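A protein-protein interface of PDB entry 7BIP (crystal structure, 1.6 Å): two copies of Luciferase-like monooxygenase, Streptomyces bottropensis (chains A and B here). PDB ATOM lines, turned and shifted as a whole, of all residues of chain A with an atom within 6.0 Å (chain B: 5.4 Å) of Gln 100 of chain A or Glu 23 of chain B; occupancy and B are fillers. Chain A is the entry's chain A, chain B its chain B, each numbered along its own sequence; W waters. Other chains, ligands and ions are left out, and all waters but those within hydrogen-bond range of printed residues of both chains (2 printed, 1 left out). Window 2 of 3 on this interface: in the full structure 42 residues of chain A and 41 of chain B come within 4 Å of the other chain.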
ATOM      1  N   LEU A  95       5.494   8.920  22.303  1.00  0.00           N
ATOM      2  CA  LEU A  95       5.415   9.048  23.756  1.00  0.00           C
ATOM      3  C   LEU A  95       4.491   7.995  24.359  1.00  0.00           C
ATOM      4  O   LEU A  95       4.793   7.440  25.422  1.00  0.00           O
ATOM      5  CB  LEU A  95       4.943  10.460  24.114  1.00  0.00           C
ATOM      6  CG  LEU A  95       4.657  10.704  25.592  1.00  0.00           C
ATOM      7  CD1 LEU A  95       5.904  10.367  26.423  1.00  0.00           C
ATOM      8  CD2 LEU A  95       4.256  12.167  25.770  1.00  0.00           C
ATOM      9  N   ASP A  96       3.357   7.714  23.704  1.00  0.00           N
ATOM     10  CA  ASP A  96       2.468   6.658  24.174  1.00  0.00           C
ATOM     11  C   ASP A  96       3.226   5.338  24.303  1.00  0.00           C
ATOM     12  O   ASP A  96       3.142   4.649  25.329  1.00  0.00           O
ATOM     13  CB  ASP A  96       1.280   6.514  23.214  1.00  0.00           C
ATOM     14  CG  ASP A  96       0.126   5.727  23.814  1.00  0.00           C
ATOM     15  OD1 ASP A  96      -0.025   5.710  25.054  1.00  0.00           O
ATOM     16  OD2 ASP A  96      -0.643   5.127  23.036  1.00  0.00           O
ATOM     17  N   ASN A  97       4.013   4.993  23.282  1.00  0.00           N
ATOM     18  CA  ASN A  97       4.763   3.740  23.319  1.00  0.00           C
ATOM     19  C   ASN A  97       5.898   3.772  24.340  1.00  0.00           C
ATOM     20  O   ASN A  97       6.107   2.793  25.065  1.00  0.00           O
ATOM     21  CB  ASN A  97       5.284   3.419  21.922  1.00  0.00           C
ATOM     22  CG  ASN A  97       4.208   2.814  21.048  1.00  0.00           C
ATOM     23  OD1 ASN A  97       3.809   1.675  21.251  1.00  0.00           O
ATOM     24  ND2 ASN A  97       3.710   3.593  20.089  1.00  0.00           N
ATOM     25  N   ILE A  98       6.639   4.880  24.413  1.00  0.00           N
ATOM     26  CA  ILE A  98       7.717   5.001  25.393  1.00  0.00           C
ATOM     27  C   ILE A  98       7.176   4.836  26.807  1.00  0.00           C
ATOM     28  O   ILE A  98       7.785   4.165  27.656  1.00  0.00           O
ATOM     29  CB  ILE A  98       8.432   6.353  25.206  1.00  0.00           C
ATOM     30  CG1 ILE A  98       9.330   6.288  23.970  1.00  0.00           C
ATOM     31  CG2 ILE A  98       9.256   6.733  26.451  1.00  0.00           C
ATOM     32  CD1 ILE A  98       9.725   7.666  23.458  1.00  0.00           C
ATOM     33  N   SER A  99       6.011   5.428  27.077  1.00  0.00           N
ATOM     34  CA  SER A  99       5.394   5.379  28.397  1.00  0.00           C
ATOM     35  C   SER A  99       4.587   4.109  28.639  1.00  0.00           C
ATOM     36  O   SER A  99       4.020   3.962  29.724  1.00  0.00           O
ATOM     37  CB  SER A  99       4.484   6.604  28.583  1.00  0.00           C
ATOM     38  OG  SER A  99       3.259   6.419  27.872  1.00  0.00           O
ATOM     39  N   GLN A 100       4.521   3.203  27.662  1.00  0.00           N
ATOM     40  CA  GLN A 100       3.761   1.947  27.769  1.00  0.00           C
ATOM     41  C   GLN A 100       2.296   2.211  28.144  1.00  0.00           C
ATOM     42  O   GLN A 100       1.718   1.597  29.051  1.00  0.00           O
ATOM     43  CB  GLN A 100       4.451   0.969  28.736  1.00  0.00           C
ATOM     44  CG  GLN A 100       5.909   0.707  28.313  1.00  0.00           C
ATOM     45  CD  GLN A 100       6.435  -0.654  28.719  1.00  0.00           C
ATOM     46  OE1 GLN A 100       5.989  -1.242  29.705  1.00  0.00           O
ATOM     47  NE2 GLN A 100       7.394  -1.166  27.950  1.00  0.00           N
ATOM     48  N   GLY A 101       1.686   3.145  27.408  1.00  0.00           N
ATOM     49  CA  GLY A 101       0.252   3.352  27.480  1.00  0.00           C
ATOM     50  C   GLY A 101      -0.240   4.260  28.584  1.00  0.00           C
ATOM     51  O   GLY A 101      -1.416   4.168  28.956  1.00  0.00           O
ATOM     52  N   ARG A 102       0.608   5.155  29.106  1.00  0.00           N
ATOM     53  CA  ARG A 102       0.245   5.997  30.244  1.00  0.00           C
ATOM     54  C   ARG A 102      -0.117   7.424  29.842  1.00  0.00           C
ATOM     55  O   ARG A 102      -0.320   8.268  30.721  1.00  0.00           O
ATOM     56  CB  ARG A 102       1.386   6.029  31.270  1.00  0.00           C
ATOM     57  CG  ARG A 102       1.613   4.703  32.004  1.00  0.00           C
ATOM     58  CD  ARG A 102       2.730   4.823  33.039  1.00  0.00           C
ATOM     59  NE  ARG A 102       4.064   4.885  32.430  1.00  0.00           N
ATOM     60  CZ  ARG A 102       5.067   5.627  32.900  1.00  0.00           C
ATOM     61  NH1 ARG A 102       4.888   6.396  33.968  1.00  0.00           N
ATOM     62  NH2 ARG A 102       6.252   5.605  32.297  1.00  0.00           N
ATOM     63  N   TRP A 165       0.149   2.936  21.300  1.00  0.00           N
ATOM     64  CA  TRP A 165       0.055   1.799  22.204  1.00  0.00           C
ATOM     65  C   TRP A 165      -1.392   1.574  22.619  1.00  0.00           C
ATOM     66  O   TRP A 165      -1.916   0.454  22.521  1.00  0.00           O
ATOM     67  CB  TRP A 165       0.940   2.073  23.420  1.00  0.00           C
ATOM     68  CG  TRP A 165       0.890   1.060  24.533  1.00  0.00           C
ATOM     69  CD1 TRP A 165      -0.178   0.770  25.348  1.00  0.00           C
ATOM     70  CD2 TRP A 165       1.973   0.245  24.991  1.00  0.00           C
ATOM     71  NE1 TRP A 165       0.180  -0.182  26.266  1.00  0.00           N
ATOM     72  CE2 TRP A 165       1.496  -0.518  26.070  1.00  0.00           C
ATOM     73  CE3 TRP A 165       3.302   0.090  24.589  1.00  0.00           C
ATOM     74  CZ2 TRP A 165       2.301  -1.441  26.750  1.00  0.00           C
ATOM     75  CZ3 TRP A 165       4.101  -0.819  25.257  1.00  0.00           C
ATOM     76  CH2 TRP A 165       3.601  -1.571  26.332  1.00  0.00           C
ATOM     77  N   ALA B  18       5.912  -1.226  17.918  1.00  0.00           N
ATOM     78  CA  ALA B  18       6.510   0.019  18.395  1.00  0.00           C
ATOM     79  C   ALA B  18       6.836  -0.068  19.880  1.00  0.00           C
ATOM     80  O   ALA B  18       7.877   0.431  20.327  1.00  0.00           O
ATOM     81  CB  ALA B  18       5.582   1.207  18.121  1.00  0.00           C
ATOM     82  N   GLY B  19       5.973  -0.723  20.656  1.00  0.00           N
ATOM     83  CA  GLY B  19       6.223  -0.822  22.083  1.00  0.00           C
ATOM     84  C   GLY B  19       7.485  -1.604  22.387  1.00  0.00           C
ATOM     85  O   GLY B  19       8.295  -1.199  23.230  1.00  0.00           O
ATOM     86  N   GLN B  20       7.679  -2.728  21.692  1.00  0.00           N
ATOM     87  CA  GLN B  20       8.906  -3.497  21.885  1.00  0.00           C
ATOM     88  C   GLN B  20      10.123  -2.710  21.415  1.00  0.00           C
ATOM     89  O   GLN B  20      11.159  -2.687  22.092  1.00  0.00           O
ATOM     90  CB  GLN B  20       8.808  -4.839  21.151  1.00  0.00           C
ATOM     91  CG  GLN B  20      10.072  -5.686  21.294  1.00  0.00           C
ATOM     92  CD  GLN B  20      10.046  -6.959  20.473  1.00  0.00           C
ATOM     93  OE1 GLN B  20       9.079  -7.237  19.762  1.00  0.00           O
ATOM     94  NE2 GLN B  20      11.121  -7.737  20.557  1.00  0.00           N
ATOM     95  N   HIS B  21      10.010  -2.034  20.271  1.00  0.00           N
ATOM     96  CA  HIS B  21      11.136  -1.267  19.747  1.00  0.00           C
ATOM     97  C   HIS B  21      11.603  -0.203  20.740  1.00  0.00           C
ATOM     98  O   HIS B  21      12.804  -0.054  20.989  1.00  0.00           O
ATOM     99  CB  HIS B  21      10.763  -0.609  18.412  1.00  0.00           C
ATOM    100  CG  HIS B  21      11.708   0.480  18.020  1.00  0.00           C
ATOM    101  ND1 HIS B  21      12.971   0.223  17.532  1.00  0.00           N
ATOM    102  CD2 HIS B  21      11.604   1.826  18.117  1.00  0.00           C
ATOM    103  CE1 HIS B  21      13.596   1.368  17.316  1.00  0.00           C
ATOM    104  NE2 HIS B  21      12.790   2.355  17.666  1.00  0.00           N
ATOM    105  N   PHE B  22      10.673   0.562  21.309  1.00  0.00           N
ATOM    106  CA  PHE B  22      11.110   1.655  22.175  1.00  0.00           C
ATOM    107  C   PHE B  22      11.646   1.130  23.499  1.00  0.00           C
ATOM    108  O   PHE B  22      12.609   1.682  24.035  1.00  0.00           O
ATOM    109  CB  PHE B  22       9.984   2.660  22.386  1.00  0.00           C
ATOM    110  CG  PHE B  22       9.803   3.558  21.214  1.00  0.00           C
ATOM    111  CD1 PHE B  22      10.783   4.477  20.878  1.00  0.00           C
ATOM    112  CD2 PHE B  22       8.693   3.430  20.397  1.00  0.00           C
ATOM    113  CE1 PHE B  22      10.629   5.296  19.768  1.00  0.00           C
ATOM    114  CE2 PHE B  22       8.536   4.231  19.295  1.00  0.00           C
ATOM    115  CZ  PHE B  22       9.503   5.164  18.971  1.00  0.00           C
ATOM    116  N   GLU B  23      11.054   0.057  24.032  1.00  0.00           N
ATOM    117  CA  GLU B  23      11.575  -0.567  25.253  1.00  0.00           C
ATOM    118  C   GLU B  23      13.001  -1.063  25.046  1.00  0.00           C
ATOM    119  O   GLU B  23      13.894  -0.835  25.876  1.00  0.00           O
ATOM    120  CB  GLU B  23      10.649  -1.718  25.670  1.00  0.00           C
ATOM    121  CG  GLU B  23      11.056  -2.509  26.907  1.00  0.00           C
ATOM    122  CD  GLU B  23      10.143  -3.715  27.156  1.00  0.00           C
ATOM    123  OE1 GLU B  23       9.631  -3.864  28.283  1.00  0.00           O
ATOM    124  OE2 GLU B  23       9.933  -4.518  26.219  1.00  0.00           O
ATOM    125  N   GLU B  24      13.235  -1.758  23.939  1.00  0.00           N
ATOM    126  CA  GLU B  24      14.563  -2.302  23.694  1.00  0.00           C
ATOM    127  C   GLU B  24      15.567  -1.206  23.350  1.00  0.00           C
ATOM    128  O   GLU B  24      16.735  -1.281  23.751  1.00  0.00           O
ATOM    129  CB  GLU B  24      14.481  -3.350  22.586  1.00  0.00           C
ATOM    130  CG  GLU B  24      13.827  -4.622  23.081  1.00  0.00           C
ATOM    131  CD  GLU B  24      13.697  -5.692  22.012  1.00  0.00           C
ATOM    132  OE1 GLU B  24      14.199  -5.499  20.876  1.00  0.00           O
ATOM    133  OE2 GLU B  24      13.086  -6.735  22.329  1.00  0.00           O
ATOM    134  N   SER B  25      15.142  -0.185  22.600  1.00  0.00           N
ATOM    135  CA  SER B  25      16.067   0.883  22.233  1.00  0.00           C
ATOM    136  C   SER B  25      16.490   1.697  23.454  1.00  0.00           C
ATOM    137  O   SER B  25      17.647   2.126  23.549  1.00  0.00           O
ATOM    138  CB  SER B  25      15.423   1.789  21.184  1.00  0.00           C
ATOM    139  OG  SER B  25      15.388   1.117  19.931  1.00  0.00           O
ATOM    140  N   LEU B  26      15.573   1.932  24.392  1.00  0.00           N
ATOM    141  CA  LEU B  26      15.977   2.618  25.614  1.00  0.00           C
ATOM    142  C   LEU B  26      16.951   1.763  26.414  1.00  0.00           C
ATOM    143  O   LEU B  26      17.883   2.291  27.028  1.00  0.00           O
ATOM    144  CB  LEU B  26      14.749   2.988  26.456  1.00  0.00           C
ATOM    145  CG  LEU B  26      13.910   4.150  25.905  1.00  0.00           C
ATOM    146  CD1 LEU B  26      12.657   4.349  26.707  1.00  0.00           C
ATOM    147  CD2 LEU B  26      14.724   5.453  25.885  1.00  0.00           C
ATOM    148  N   ARG B  27      16.776   0.435  26.395  1.00  0.00           N
ATOM    149  CA  ARG B  27      17.726  -0.410  27.111  1.00  0.00           C
ATOM    150  C   ARG B  27      19.085  -0.432  26.417  1.00  0.00           C
ATOM    151  O   ARG B  27      20.119  -0.543  27.088  1.00  0.00           O
ATOM    152  CB  ARG B  27      17.189  -1.831  27.253  1.00  0.00           C
ATOM    153  CG  ARG B  27      17.861  -2.580  28.377  1.00  0.00           C
ATOM    154  CD  ARG B  27      16.881  -3.498  29.079  1.00  0.00           C
ATOM    155  NE  ARG B  27      16.727  -4.735  28.336  1.00  0.00           N
ATOM    156  CZ  ARG B  27      17.617  -5.720  28.341  1.00  0.00           C
ATOM    157  NH1 ARG B  27      18.725  -5.610  29.064  1.00  0.00           N
ATOM    158  NH2 ARG B  27      17.390  -6.821  27.641  1.00  0.00           N
ATOM    159  N   LEU B  28      19.105  -0.332  25.080  1.00  0.00           N
ATOM    160  CA  LEU B  28      20.377  -0.209  24.375  1.00  0.00           C
ATOM    161  C   LEU B  28      21.062   1.117  24.699  1.00  0.00           C
ATOM    162  O   LEU B  28      22.297   1.176  24.764  1.00  0.00           O
ATOM    163  CB  LEU B  28      20.159  -0.350  22.863  1.00  0.00           C
ATOM    164  CG  LEU B  28      19.811  -1.776  22.409  1.00  0.00           C
ATOM    165  CD1 LEU B  28      19.352  -1.739  20.948  1.00  0.00           C
ATOM    166  CD2 LEU B  28      21.008  -2.743  22.587  1.00  0.00           C
HETATM  167  O   HOH W   1       3.029  -0.816  20.389  1.00  0.00           O
HETATM  168  O   HOH W   2       7.788   0.574  25.331  1.00  0.00           O
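The side-chain amide oxygen (OD1) of Asn 97 of chain A lies within hydrogen-bond range of the backbone NH (N) of Gly 19 of chain B.
The backbone NH (N) of Trp 165 of chain A lies within hydrogen-bond range of the side-chain carboxylate (OD2) of Asp 96 of chain A (2.9 Å).
Asn 97 of chain A touches Ala 18 of chain B. Asn 97 of chain A touches Phe 22 of chain B (CB to CD2, 3.7 Å). CD1 of Phe 22 of chain B touches CG1 of Ile 98 of chain A, at 3.9 Å. Gln 100 of chain A touches Glu 23 of chain B. Gly 19 of chain B touches Trp 165 of chain A (CA to CZ3, 3.8 Å).
Of the printed residues of chain B, Gln 100 of chain A touches Glu 23. Printed residues of chain A within 4 Å of Glu 23 of chain B: Gln 100. Printed residues of chain B within 4 Å of Asn 97 of chain A: Ala 18 (3.6 Å), Gly 19 (3.3 Å) and Phe 22 (3.7 Å). Printed residues of chain A within 4 Å of Phe 22 of chain B: Asn 97 (3.7 Å) and Ile 98 (3.9 Å). Gly 101 of chain A touches none of the printed residues of chain B. The nearest printed residue of chain A that does not touch Ala 18 of chain B is Trp 165 of chain A (5.9 Å).
Hydrophobic or aromatic side chains of chain A within 4 Å of the printed part of chain B: Ile 98 and Trp 165. Among the printed residues, no Asp or Glu carboxylate lies within 4 Å of a Lys or Arg side-chain nitrogen of the other chain.
No position is printed for both chains. Of the 6 pairs that touch across the chains among the printed residues, none has its exchanged pair printed and touching as well.
Water W1 bridges OD1 of Asn 97 of chain A (2.7 Å) and N of Gly 19 of chain B (3.0 Å). Water W2 lies within hydrogen-bond range of the backbone carbonyl oxygen of Asn 97 of chain A (2.8 Å), the backbone carbonyl oxygen of Gly 19 of chain B (2.8 Å) and the side-chain amide nitrogen of Gln 100 of chain A (3.2 Å).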
